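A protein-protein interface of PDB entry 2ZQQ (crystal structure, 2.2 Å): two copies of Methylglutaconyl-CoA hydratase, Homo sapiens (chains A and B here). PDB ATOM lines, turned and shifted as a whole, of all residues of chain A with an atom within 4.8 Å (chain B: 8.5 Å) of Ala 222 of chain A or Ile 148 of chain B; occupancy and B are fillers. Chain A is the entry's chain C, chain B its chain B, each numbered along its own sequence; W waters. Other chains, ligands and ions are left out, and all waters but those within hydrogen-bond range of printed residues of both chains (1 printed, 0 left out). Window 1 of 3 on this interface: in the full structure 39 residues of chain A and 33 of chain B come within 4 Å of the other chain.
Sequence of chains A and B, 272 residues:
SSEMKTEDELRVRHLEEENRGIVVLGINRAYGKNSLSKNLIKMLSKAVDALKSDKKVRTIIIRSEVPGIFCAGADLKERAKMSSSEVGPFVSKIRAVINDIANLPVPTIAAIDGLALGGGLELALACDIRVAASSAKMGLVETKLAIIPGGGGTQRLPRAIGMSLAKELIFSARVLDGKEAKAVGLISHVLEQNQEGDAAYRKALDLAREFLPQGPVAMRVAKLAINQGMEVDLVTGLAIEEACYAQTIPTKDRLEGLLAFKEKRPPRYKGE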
ATOM      1  N   ALA A 218     -21.783   7.737  10.464  1.00  0.00           N
ATOM      2  CA  ALA A 218     -22.434   6.467  10.163  1.00  0.00           C
ATOM      3  C   ALA A 218     -21.958   5.372  11.114  1.00  0.00           C
ATOM      4  O   ALA A 218     -22.759   4.576  11.605  1.00  0.00           O
ATOM      5  CB  ALA A 218     -22.153   6.054   8.707  1.00  0.00           C
ATOM      6  N   MET A 219     -20.652   5.340  11.367  1.00  0.00           N
ATOM      7  CA  MET A 219     -20.062   4.343  12.262  1.00  0.00           C
ATOM      8  C   MET A 219     -20.610   4.449  13.679  1.00  0.00           C
ATOM      9  O   MET A 219     -20.855   3.435  14.329  1.00  0.00           O
ATOM     10  CB  MET A 219     -18.530   4.485  12.300  1.00  0.00           C
ATOM     11  CG  MET A 219     -17.859   4.177  10.970  1.00  0.00           C
ATOM     12  SD  MET A 219     -17.975   2.419  10.513  1.00  0.00           S
ATOM     13  CE  MET A 219     -16.373   1.822  11.120  1.00  0.00           C
ATOM     14  N   ARG A 220     -20.795   5.676  14.154  1.00  0.00           N
ATOM     15  CA  ARG A 220     -21.310   5.887  15.496  1.00  0.00           C
ATOM     16  C   ARG A 220     -22.768   5.494  15.643  1.00  0.00           C
ATOM     17  O   ARG A 220     -23.110   4.776  16.577  1.00  0.00           O
ATOM     18  CB  ARG A 220     -21.128   7.347  15.925  1.00  0.00           C
ATOM     19  CG  ARG A 220     -19.724   7.664  16.441  1.00  0.00           C
ATOM     20  CD  ARG A 220     -19.444   9.161  16.409  1.00  0.00           C
ATOM     21  NE  ARG A 220     -18.040   9.465  16.691  1.00  0.00           N
ATOM     22  CZ  ARG A 220     -17.540   9.656  17.909  1.00  0.00           C
ATOM     23  NH1 ARG A 220     -18.330   9.579  18.973  1.00  0.00           N
ATOM     24  NH2 ARG A 220     -16.249   9.929  18.062  1.00  0.00           N
ATOM     25  N   VAL A 221     -23.633   5.956  14.742  1.00  0.00           N
ATOM     26  CA  VAL A 221     -25.046   5.612  14.865  1.00  0.00           C
ATOM     27  C   VAL A 221     -25.286   4.145  14.560  1.00  0.00           C
ATOM     28  O   VAL A 221     -26.286   3.587  14.990  1.00  0.00           O
ATOM     29  CB  VAL A 221     -25.973   6.498  13.970  1.00  0.00           C
ATOM     30  CG1 VAL A 221     -25.869   7.941  14.417  1.00  0.00           C
ATOM     31  CG2 VAL A 221     -25.624   6.348  12.497  1.00  0.00           C
ATOM     32  N   ALA A 222     -24.358   3.519  13.836  1.00  0.00           N
ATOM     33  CA  ALA A 222     -24.482   2.095  13.512  1.00  0.00           C
ATOM     34  C   ALA A 222     -24.237   1.277  14.783  1.00  0.00           C
ATOM     35  O   ALA A 222     -24.953   0.307  15.058  1.00  0.00           O
ATOM     36  CB  ALA A 222     -23.477   1.707  12.438  1.00  0.00           C
ATOM     37  N   LYS A 223     -23.225   1.662  15.561  1.00  0.00           N
ATOM     38  CA  LYS A 223     -22.953   0.937  16.793  1.00  0.00           C
ATOM     39  C   LYS A 223     -24.115   1.189  17.743  1.00  0.00           C
ATOM     40  O   LYS A 223     -24.522   0.306  18.493  1.00  0.00           O
ATOM     41  CB  LYS A 223     -21.636   1.390  17.442  1.00  0.00           C
ATOM     42  CG  LYS A 223     -21.342   0.631  18.733  1.00  0.00           C
ATOM     43  CD  LYS A 223     -19.952   0.920  19.308  1.00  0.00           C
ATOM     44  CE  LYS A 223     -19.774   0.202  20.647  1.00  0.00           C
ATOM     45  NZ  LYS A 223     -18.367   0.227  21.153  1.00  0.00           N
ATOM     46  N   LEU A 224     -24.646   2.407  17.700  1.00  0.00           N
ATOM     47  CA  LEU A 224     -25.781   2.781  18.528  1.00  0.00           C
ATOM     48  C   LEU A 224     -26.974   1.898  18.139  1.00  0.00           C
ATOM     49  O   LEU A 224     -27.633   1.299  18.990  1.00  0.00           O
ATOM     50  CB  LEU A 224     -26.112   4.266  18.306  1.00  0.00           C
ATOM     51  CG  LEU A 224     -27.371   4.853  18.957  1.00  0.00           C
ATOM     52  CD1 LEU A 224     -27.278   4.735  20.467  1.00  0.00           C
ATOM     53  CD2 LEU A 224     -27.512   6.312  18.562  1.00  0.00           C
ATOM     54  N   ALA A 225     -27.240   1.808  16.842  1.00  0.00           N
ATOM     55  CA  ALA A 225     -28.352   0.997  16.355  1.00  0.00           C
ATOM     56  C   ALA A 225     -28.232  -0.466  16.802  1.00  0.00           C
ATOM     57  O   ALA A 225     -29.184  -1.056  17.317  1.00  0.00           O
ATOM     58  CB  ALA A 225     -28.423   1.078  14.827  1.00  0.00           C
ATOM     59  N   ILE A 226     -27.054  -1.048  16.612  1.00  0.00           N
ATOM     60  CA  ILE A 226     -26.843  -2.434  16.994  1.00  0.00           C
ATOM     61  C   ILE A 226     -26.982  -2.645  18.509  1.00  0.00           C
ATOM     62  O   ILE A 226     -27.796  -3.455  18.950  1.00  0.00           O
ATOM     63  CB  ILE A 226     -25.451  -2.928  16.512  1.00  0.00           C
ATOM     64  CG1 ILE A 226     -25.389  -2.873  14.982  1.00  0.00           C
ATOM     65  CG2 ILE A 226     -25.212  -4.365  16.977  1.00  0.00           C
ATOM     66  CD1 ILE A 226     -23.975  -2.985  14.412  1.00  0.00           C
ATOM     67  N   GLU A 241     -33.253   1.659  14.297  1.00  0.00           N
ATOM     68  CA  GLU A 241     -32.445   1.723  13.087  1.00  0.00           C
ATOM     69  C   GLU A 241     -32.877   2.957  12.276  1.00  0.00           C
ATOM     70  O   GLU A 241     -32.040   3.718  11.783  1.00  0.00           O
ATOM     71  CB  GLU A 241     -32.624   0.462  12.236  1.00  0.00           C
ATOM     72  CG  GLU A 241     -31.908   0.558  10.895  1.00  0.00           C
ATOM     73  CD  GLU A 241     -32.072  -0.692  10.041  1.00  0.00           C
ATOM     74  OE1 GLU A 241     -31.498  -1.746  10.400  1.00  0.00           O
ATOM     75  OE2 GLU A 241     -32.779  -0.612   9.012  1.00  0.00           O
ATOM     76  N   CYS A 244     -31.458   6.140  13.722  1.00  0.00           N
ATOM     77  CA  CYS A 244     -30.026   6.216  13.463  1.00  0.00           C
ATOM     78  C   CYS A 244     -29.748   6.567  12.004  1.00  0.00           C
ATOM     79  O   CYS A 244     -28.949   7.464  11.711  1.00  0.00           O
ATOM     80  CB  CYS A 244     -29.364   4.895  13.840  1.00  0.00           C
ATOM     81  SG  CYS A 244     -29.394   4.617  15.645  1.00  0.00           S
ATOM     82  N   TYR A 245     -30.429   5.882  11.093  1.00  0.00           N
ATOM     83  CA  TYR A 245     -30.252   6.137   9.676  1.00  0.00           C
ATOM     84  C   TYR A 245     -30.548   7.601   9.386  1.00  0.00           C
ATOM     85  O   TYR A 245     -29.824   8.251   8.625  1.00  0.00           O
ATOM     86  CB  TYR A 245     -31.203   5.254   8.849  1.00  0.00           C
ATOM     87  CG  TYR A 245     -30.939   5.284   7.360  1.00  0.00           C
ATOM     88  CD1 TYR A 245     -30.102   4.347   6.760  1.00  0.00           C
ATOM     89  CD2 TYR A 245     -31.512   6.265   6.551  1.00  0.00           C
ATOM     90  CE1 TYR A 245     -29.839   4.390   5.377  1.00  0.00           C
ATOM     91  CE2 TYR A 245     -31.260   6.318   5.177  1.00  0.00           C
ATOM     92  CZ  TYR A 245     -30.421   5.383   4.598  1.00  0.00           C
ATOM     93  OH  TYR A 245     -30.149   5.455   3.250  1.00  0.00           O
ATOM     94  N   THR A 248     -27.800  10.175   9.309  1.00  0.00           N
ATOM     95  CA  THR A 248     -26.835  10.254   8.211  1.00  0.00           C
ATOM     96  C   THR A 248     -27.380  10.972   6.980  1.00  0.00           C
ATOM     97  O   THR A 248     -26.615  11.437   6.134  1.00  0.00           O
ATOM     98  CB  THR A 248     -26.385   8.859   7.759  1.00  0.00           C
ATOM     99  OG1 THR A 248     -27.511   8.149   7.227  1.00  0.00           O
ATOM    100  CG2 THR A 248     -25.804   8.073   8.926  1.00  0.00           C
ATOM    101  N   ARG B  79     -31.440   7.127  -5.835  1.00  0.00           N
ATOM    102  CA  ARG B  79     -30.998   7.799  -4.620  1.00  0.00           C
ATOM    103  C   ARG B  79     -30.300   9.117  -4.935  1.00  0.00           C
ATOM    104  O   ARG B  79     -30.431  10.088  -4.189  1.00  0.00           O
ATOM    105  CB  ARG B  79     -30.051   6.899  -3.814  1.00  0.00           C
ATOM    106  CG  ARG B  79     -29.786   7.398  -2.393  1.00  0.00           C
ATOM    107  CD  ARG B  79     -31.081   7.446  -1.592  1.00  0.00           C
ATOM    108  NE  ARG B  79     -31.730   6.137  -1.560  1.00  0.00           N
ATOM    109  CZ  ARG B  79     -31.346   5.127  -0.788  1.00  0.00           C
ATOM    110  NH1 ARG B  79     -30.314   5.273   0.034  1.00  0.00           N
ATOM    111  NH2 ARG B  79     -31.980   3.964  -0.852  1.00  0.00           N
ATOM    112  N   VAL B  91     -36.496   4.769   2.221  1.00  0.00           N
ATOM    113  CA  VAL B  91     -35.754   3.726   2.916  1.00  0.00           C
ATOM    114  C   VAL B  91     -36.656   3.014   3.933  1.00  0.00           C
ATOM    115  O   VAL B  91     -36.505   1.821   4.165  1.00  0.00           O
ATOM    116  CB  VAL B  91     -34.503   4.315   3.622  1.00  0.00           C
ATOM    117  CG1 VAL B  91     -33.837   3.251   4.493  1.00  0.00           C
ATOM    118  CG2 VAL B  91     -33.503   4.833   2.566  1.00  0.00           C
ATOM    119  N   ARG B  95     -37.591  -0.874   4.335  1.00  0.00           N
ATOM    120  CA  ARG B  95     -37.476  -1.556   5.616  1.00  0.00           C
ATOM    121  C   ARG B  95     -38.779  -2.296   5.911  1.00  0.00           C
ATOM    122  O   ARG B  95     -38.756  -3.460   6.325  1.00  0.00           O
ATOM    123  CB  ARG B  95     -37.176  -0.550   6.742  1.00  0.00           C
ATOM    124  CG  ARG B  95     -36.923  -1.203   8.106  1.00  0.00           C
ATOM    125  CD  ARG B  95     -36.542  -0.172   9.199  1.00  0.00           C
ATOM    126  NE  ARG B  95     -35.426   0.687   8.799  1.00  0.00           N
ATOM    127  CZ  ARG B  95     -35.538   1.977   8.491  1.00  0.00           C
ATOM    128  NH1 ARG B  95     -36.717   2.591   8.536  1.00  0.00           N
ATOM    129  NH2 ARG B  95     -34.468   2.651   8.107  1.00  0.00           N
ATOM    130  N   GLY B 118     -26.245  -4.606   0.624  1.00  0.00           N
ATOM    131  CA  GLY B 118     -27.195  -3.748   1.309  1.00  0.00           C
ATOM    132  C   GLY B 118     -28.570  -4.361   1.393  1.00  0.00           C
ATOM    133  O   GLY B 118     -28.726  -5.494   1.856  1.00  0.00           O
ATOM    134  N   GLY B 119     -29.572  -3.615   0.937  1.00  0.00           N
ATOM    135  CA  GLY B 119     -30.935  -4.115   0.957  1.00  0.00           C
ATOM    136  C   GLY B 119     -31.030  -5.543   0.455  1.00  0.00           C
ATOM    137  O   GLY B 119     -31.903  -6.300   0.888  1.00  0.00           O
ATOM    138  N   GLU B 122     -30.112  -7.746   3.301  1.00  0.00           N
ATOM    139  CA  GLU B 122     -31.125  -7.538   4.338  1.00  0.00           C
ATOM    140  C   GLU B 122     -32.411  -8.277   4.007  1.00  0.00           C
ATOM    141  O   GLU B 122     -33.124  -8.759   4.895  1.00  0.00           O
ATOM    142  CB  GLU B 122     -31.411  -6.058   4.484  1.00  0.00           C
ATOM    143  CG  GLU B 122     -30.216  -5.292   4.971  1.00  0.00           C
ATOM    144  CD  GLU B 122     -30.478  -3.825   5.008  1.00  0.00           C
ATOM    145  OE1 GLU B 122     -30.306  -3.221   6.093  1.00  0.00           O
ATOM    146  OE2 GLU B 122     -30.858  -3.278   3.946  1.00  0.00           O
ATOM    147  N   LEU B 140     -22.827  -5.924   3.935  1.00  0.00           N
ATOM    148  CA  LEU B 140     -23.507  -4.661   4.192  1.00  0.00           C
ATOM    149  C   LEU B 140     -22.370  -3.646   4.163  1.00  0.00           C
ATOM    150  O   LEU B 140     -21.588  -3.551   5.106  1.00  0.00           O
ATOM    151  CB  LEU B 140     -24.198  -4.683   5.566  1.00  0.00           C
ATOM    152  CG  LEU B 140     -25.337  -5.690   5.770  1.00  0.00           C
ATOM    153  CD1 LEU B 140     -25.868  -5.603   7.195  1.00  0.00           C
ATOM    154  CD2 LEU B 140     -26.450  -5.417   4.781  1.00  0.00           C
ATOM    155  N   VAL B 141     -22.274  -2.904   3.064  1.00  0.00           N
ATOM    156  CA  VAL B 141     -21.201  -1.934   2.884  1.00  0.00           C
ATOM    157  C   VAL B 141     -21.612  -0.479   3.123  1.00  0.00           C
ATOM    158  O   VAL B 141     -20.846   0.451   2.835  1.00  0.00           O
ATOM    159  CB  VAL B 141     -20.622  -2.062   1.458  1.00  0.00           C
ATOM    160  CG1 VAL B 141     -20.178  -3.498   1.211  1.00  0.00           C
ATOM    161  CG2 VAL B 141     -21.669  -1.663   0.430  1.00  0.00           C
ATOM    162  N   GLU B 142     -22.811  -0.294   3.660  1.00  0.00           N
ATOM    163  CA  GLU B 142     -23.343   1.034   3.925  1.00  0.00           C
ATOM    164  C   GLU B 142     -22.415   2.068   4.585  1.00  0.00           C
ATOM    165  O   GLU B 142     -22.385   3.223   4.170  1.00  0.00           O
ATOM    166  CB  GLU B 142     -24.634   0.918   4.742  1.00  0.00           C
ATOM    167  CG  GLU B 142     -25.866   0.509   3.937  1.00  0.00           C
ATOM    168  CD  GLU B 142     -25.939  -0.988   3.659  1.00  0.00           C
ATOM    169  OE1 GLU B 142     -25.279  -1.774   4.366  1.00  0.00           O
ATOM    170  OE2 GLU B 142     -26.683  -1.387   2.738  1.00  0.00           O
ATOM    171  N   THR B 143     -21.670   1.682   5.608  1.00  0.00           N
ATOM    172  CA  THR B 143     -20.796   2.654   6.261  1.00  0.00           C
ATOM    173  C   THR B 143     -19.736   3.207   5.312  1.00  0.00           C
ATOM    174  O   THR B 143     -19.173   4.275   5.558  1.00  0.00           O
ATOM    175  CB  THR B 143     -20.101   2.055   7.498  1.00  0.00           C
ATOM    176  OG1 THR B 143     -19.381   0.876   7.117  1.00  0.00           O
ATOM    177  CG2 THR B 143     -21.125   1.715   8.577  1.00  0.00           C
ATOM    178  N   LYS B 144     -19.461   2.488   4.227  1.00  0.00           N
ATOM    179  CA  LYS B 144     -18.480   2.955   3.255  1.00  0.00           C
ATOM    180  C   LYS B 144     -19.088   4.082   2.428  1.00  0.00           C
ATOM    181  O   LYS B 144     -18.379   4.859   1.773  1.00  0.00           O
ATOM    182  CB  LYS B 144     -18.033   1.811   2.340  1.00  0.00           C
ATOM    183  CG  LYS B 144     -16.741   1.142   2.797  1.00  0.00           C
ATOM    184  CD  LYS B 144     -16.231   0.148   1.763  1.00  0.00           C
ATOM    185  CE  LYS B 144     -14.708  -0.030   1.846  1.00  0.00           C
ATOM    186  NZ  LYS B 144     -14.220  -0.494   3.177  1.00  0.00           N
ATOM    187  N   LEU B 145     -20.409   4.172   2.478  1.00  0.00           N
ATOM    188  CA  LEU B 145     -21.135   5.207   1.763  1.00  0.00           C
ATOM    189  C   LEU B 145     -21.590   6.289   2.742  1.00  0.00           C
ATOM    190  O   LEU B 145     -22.325   7.205   2.383  1.00  0.00           O
ATOM    191  CB  LEU B 145     -22.331   4.584   1.048  1.00  0.00           C
ATOM    192  CG  LEU B 145     -21.960   3.590  -0.057  1.00  0.00           C
ATOM    193  CD1 LEU B 145     -23.162   2.730  -0.444  1.00  0.00           C
ATOM    194  CD2 LEU B 145     -21.448   4.371  -1.256  1.00  0.00           C
ATOM    195  N   ALA B 146     -21.125   6.176   3.981  1.00  0.00           N
ATOM    196  CA  ALA B 146     -21.461   7.113   5.044  1.00  0.00           C
ATOM    197  C   ALA B 146     -22.912   7.013   5.534  1.00  0.00           C
ATOM    198  O   ALA B 146     -23.475   7.979   6.048  1.00  0.00           O
ATOM    199  CB  ALA B 146     -21.137   8.540   4.609  1.00  0.00           C
ATOM    200  N   ILE B 147     -23.529   5.847   5.352  1.00  0.00           N
ATOM    201  CA  ILE B 147     -24.878   5.629   5.857  1.00  0.00           C
ATOM    202  C   ILE B 147     -24.796   4.306   6.619  1.00  0.00           C
ATOM    203  O   ILE B 147     -23.695   3.789   6.819  1.00  0.00           O
ATOM    204  CB  ILE B 147     -25.924   5.534   4.716  1.00  0.00           C
ATOM    205  CG1 ILE B 147     -25.492   4.494   3.686  1.00  0.00           C
ATOM    206  CG2 ILE B 147     -26.112   6.901   4.068  1.00  0.00           C
ATOM    207  CD1 ILE B 147     -26.523   4.264   2.587  1.00  0.00           C
ATOM    208  N   ILE B 148     -25.928   3.768   7.071  1.00  0.00           N
ATOM    209  CA  ILE B 148     -25.899   2.485   7.766  1.00  0.00           C
ATOM    210  C   ILE B 148     -26.926   1.565   7.120  1.00  0.00           C
ATOM    211  O   ILE B 148     -27.746   2.017   6.326  1.00  0.00           O
ATOM    212  CB  ILE B 148     -26.234   2.626   9.261  1.00  0.00           C
ATOM    213  CG1 ILE B 148     -27.674   3.122   9.431  1.00  0.00           C
ATOM    214  CG2 ILE B 148     -25.232   3.582   9.928  1.00  0.00           C
ATOM    215  CD1 ILE B 148     -28.212   3.004  10.856  1.00  0.00           C
ATOM    216  N   PRO B 149     -26.878   0.258   7.424  1.00  0.00           N
ATOM    217  CA  PRO B 149     -27.874  -0.634   6.809  1.00  0.00           C
ATOM    218  C   PRO B 149     -29.253  -0.138   7.240  1.00  0.00           C
ATOM    219  O   PRO B 149     -29.518  -0.002   8.439  1.00  0.00           O
ATOM    220  CB  PRO B 149     -27.530  -2.000   7.398  1.00  0.00           C
ATOM    221  CG  PRO B 149     -26.030  -1.906   7.582  1.00  0.00           C
ATOM    222  CD  PRO B 149     -25.866  -0.508   8.172  1.00  0.00           C
ATOM    223  N   GLY B 150     -30.119   0.142   6.270  1.00  0.00           N
ATOM    224  CA  GLY B 150     -31.433   0.656   6.595  1.00  0.00           C
ATOM    225  C   GLY B 150     -32.610  -0.237   6.275  1.00  0.00           C
ATOM    226  O   GLY B 150     -33.761   0.198   6.376  1.00  0.00           O
ATOM    227  N   GLY B 151     -32.344  -1.481   5.896  1.00  0.00           N
ATOM    228  CA  GLY B 151     -33.436  -2.386   5.597  1.00  0.00           C
ATOM    229  C   GLY B 151     -33.641  -3.391   6.716  1.00  0.00           C
ATOM    230  O   GLY B 151     -34.251  -4.443   6.499  1.00  0.00           O
ATOM    231  N   GLY B 152     -33.128  -3.065   7.906  1.00  0.00           N
ATOM    232  CA  GLY B 152     -33.242  -3.942   9.060  1.00  0.00           C
ATOM    233  C   GLY B 152     -31.945  -4.663   9.416  1.00  0.00           C
ATOM    234  O   GLY B 152     -31.882  -5.395  10.407  1.00  0.00           O
ATOM    235  N   GLY B 153     -30.902  -4.442   8.619  1.00  0.00           N
ATOM    236  CA  GLY B 153     -29.624  -5.095   8.849  1.00  0.00           C
ATOM    237  C   GLY B 153     -28.969  -4.876  10.209  1.00  0.00           C
ATOM    238  O   GLY B 153     -28.412  -5.814  10.786  1.00  0.00           O
ATOM    239  N   THR B 154     -29.015  -3.652  10.726  1.00  0.00           N
ATOM    240  CA  THR B 154     -28.409  -3.386  12.030  1.00  0.00           C
ATOM    241  C   THR B 154     -29.131  -4.228  13.080  1.00  0.00           C
ATOM    242  O   THR B 154     -28.619  -4.453  14.178  1.00  0.00           O
ATOM    243  CB  THR B 154     -28.530  -1.893  12.438  1.00  0.00           C
ATOM    244  OG1 THR B 154     -29.910  -1.551  12.631  1.00  0.00           O
ATOM    245  CG2 THR B 154     -27.937  -1.000  11.368  1.00  0.00           C
ATOM    246  N   GLN B 155     -30.322  -4.697  12.728  1.00  0.00           N
ATOM    247  CA  GLN B 155     -31.131  -5.494  13.644  1.00  0.00           C
ATOM    248  C   GLN B 155     -31.066  -6.993  13.405  1.00  0.00           C
ATOM    249  O   GLN B 155     -30.892  -7.760  14.351  1.00  0.00           O
ATOM    250  CB  GLN B 155     -32.596  -5.047  13.582  1.00  0.00           C
ATOM    251  CG  GLN B 155     -32.791  -3.618  13.996  1.00  0.00           C
ATOM    252  CD  GLN B 155     -32.099  -3.302  15.305  1.00  0.00           C
ATOM    253  OE1 GLN B 155     -32.414  -3.886  16.343  1.00  0.00           O
ATOM    254  NE2 GLN B 155     -31.144  -2.367  15.264  1.00  0.00           N
ATOM    255  N   PRO B 158     -27.076  -8.987  13.473  1.00  0.00           N
ATOM    256  CA  PRO B 158     -26.636  -9.268  14.847  1.00  0.00           C
ATOM    257  C   PRO B 158     -27.409 -10.427  15.483  1.00  0.00           C
ATOM    258  O   PRO B 158     -26.848 -11.233  16.230  1.00  0.00           O
ATOM    259  CB  PRO B 158     -26.920  -7.954  15.572  1.00  0.00           C
ATOM    260  CG  PRO B 158     -26.847  -6.946  14.488  1.00  0.00           C
ATOM    261  CD  PRO B 158     -27.556  -7.601  13.364  1.00  0.00           C
ATOM    262  N   ALA B 166     -21.366  -9.336  13.640  1.00  0.00           N
ATOM    263  CA  ALA B 166     -22.203  -8.372  12.945  1.00  0.00           C
ATOM    264  C   ALA B 166     -21.536  -7.002  12.948  1.00  0.00           C
ATOM    265  O   ALA B 166     -21.485  -6.331  11.918  1.00  0.00           O
ATOM    266  CB  ALA B 166     -23.572  -8.295  13.606  1.00  0.00           C
ATOM    267  N   LYS B 167     -21.034  -6.580  14.107  1.00  0.00           N
ATOM    268  CA  LYS B 167     -20.363  -5.287  14.185  1.00  0.00           C
ATOM    269  C   LYS B 167     -19.129  -5.269  13.296  1.00  0.00           C
ATOM    270  O   LYS B 167     -18.885  -4.286  12.599  1.00  0.00           O
ATOM    271  CB  LYS B 167     -19.939  -4.960  15.620  1.00  0.00           C
ATOM    272  CG  LYS B 167     -21.063  -4.530  16.539  1.00  0.00           C
ATOM    273  CD  LYS B 167     -20.546  -4.379  17.973  1.00  0.00           C
ATOM    274  CE  LYS B 167     -21.676  -4.103  18.934  1.00  0.00           C
ATOM    275  NZ  LYS B 167     -21.188  -3.948  20.328  1.00  0.00           N
ATOM    276  N   ILE B 170     -20.264  -4.813   9.713  1.00  0.00           N
ATOM    277  CA  ILE B 170     -20.837  -3.491   9.451  1.00  0.00           C
ATOM    278  C   ILE B 170     -19.767  -2.390   9.564  1.00  0.00           C
ATOM    279  O   ILE B 170     -19.725  -1.478   8.737  1.00  0.00           O
ATOM    280  CB  ILE B 170     -22.041  -3.201  10.408  1.00  0.00           C
ATOM    281  CG1 ILE B 170     -23.223  -4.089  10.009  1.00  0.00           C
ATOM    282  CG2 ILE B 170     -22.447  -1.722  10.352  1.00  0.00           C
ATOM    283  CD1 ILE B 170     -24.388  -4.069  10.988  1.00  0.00           C
ATOM    284  N   PHE B 171     -18.898  -2.495  10.568  1.00  0.00           N
ATOM    285  CA  PHE B 171     -17.822  -1.519  10.786  1.00  0.00           C
ATOM    286  C   PHE B 171     -16.786  -1.538   9.652  1.00  0.00           C
ATOM    287  O   PHE B 171     -16.251  -0.498   9.276  1.00  0.00           O
ATOM    288  CB  PHE B 171     -17.096  -1.804  12.114  1.00  0.00           C
ATOM    289  CG  PHE B 171     -17.898  -1.471  13.349  1.00  0.00           C
ATOM    290  CD1 PHE B 171     -17.565  -2.037  14.573  1.00  0.00           C
ATOM    291  CD2 PHE B 171     -18.975  -0.586  13.295  1.00  0.00           C
ATOM    292  CE1 PHE B 171     -18.287  -1.735  15.730  1.00  0.00           C
ATOM    293  CE2 PHE B 171     -19.704  -0.275  14.443  1.00  0.00           C
ATOM    294  CZ  PHE B 171     -19.359  -0.854  15.667  1.00  0.00           C
HETATM  295  O   HOH W   1     -30.057   3.284   1.820  1.00  0.00           O
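No position is printed for both chains.
Of the 30 pairs that touch across the chains among the printed residues, none has its exchanged pair printed and touching as well.
OH of Tyr 245 of chain A lies within hydrogen-bond range of NH1 of Arg 79 of chain B.
The guanidinium group of Arg 95 of chain B lies within salt-bridge range of the side-chain carboxylate of Glu 241 of chain A (3.0 Å).
OE2 of Glu 241 of chain A lies within hydrogen-bond range of N of Gly 151 of chain B, at 3.3 Å.
The backbone NH (N) of Gly 152 of chain B is in hydrogen-bond range of the side-chain carboxylate (OE2) of Glu 241 of chain A.
The side-chain carboxylate of Glu 241 of chain A sits at hydrogen-bond distance from the backbone NH of Gly 153 of chain B, 3.3 Å away.
OG1 of Thr 154 of chain B sits at hydrogen-bond distance from OE1 of Glu 241 of chain A.
The side-chain amide nitrogen of Gln 155 of chain B is in hydrogen-bond range of the backbone carbonyl oxygen of Ala 225 of chain A, at 3.1 Å.
SD of Met 219 of chain A sits close to O of Phe 171 of chain B, at 3.6 Å.
The side-chain carboxylate (OE1) of Glu 241 of chain A sits close to the backbone carbonyl oxygen (O) of Pro 149 of chain B (3.3 Å).
The side-chain carboxylate (OE2) of Glu 241 of chain A lies close to the backbone carbonyl oxygen (O) of Gly 150 of chain B, at 2.9 Å.
N of Gly 152 of chain B sits at hydrogen-bond distance from OE1 of Glu 122 of chain B (3.4 Å).
OE1 of Glu 122 of chain B is in hydrogen-bond range of N of Gly 153 of chain B, at 2.9 Å.
Of the 27 printed residues of chain B, 18 touch a printed residue of chain A.
Printed residues of chain A that touch a printed residue of chain B: Ala 218, Met 219, Val 221, Ala 222, Lys 223, Ala 225, Ile 226, Glu 241, Cys 244, Tyr 245 and Thr 248.
Hydrophobic or aromatic side chains of chain A within 4 Å of the printed part of chain B: Ala 218, Met 219, Val 221, Ala 222, Ala 225, Ile 226 and Tyr 245.
Among the printed residues, Asp or Glu carboxylates within 4 Å of a Lys or Arg side-chain nitrogen of the other chain: Glu 241 of chain A with Arg 95 of chain B.
Of chain B, only Ile 148 comes within 4 Å of Ala 222 of chain A.
Printed residues of chain A within 4 Å of Gly 150 of chain B: Glu 241 and Tyr 245.
Of the printed residues of chain B, Thr 248 of chain A touches Ala 146 (3.5 Å) and Ile 147 (3.7 Å).
The nearest residue of chain B that does not touch Ala 222 of chain A is Ile 170 of chain B (4.1 Å).
The nearest printed residue of chain A that does not touch Ile 148 of chain B is Glu 241 of chain A (4.003 Å).
Water W1 lies within hydrogen-bond range of OH of Tyr 245 of chain A (2.6 Å) and NH1 of Arg 79 of chain B (2.7 Å).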
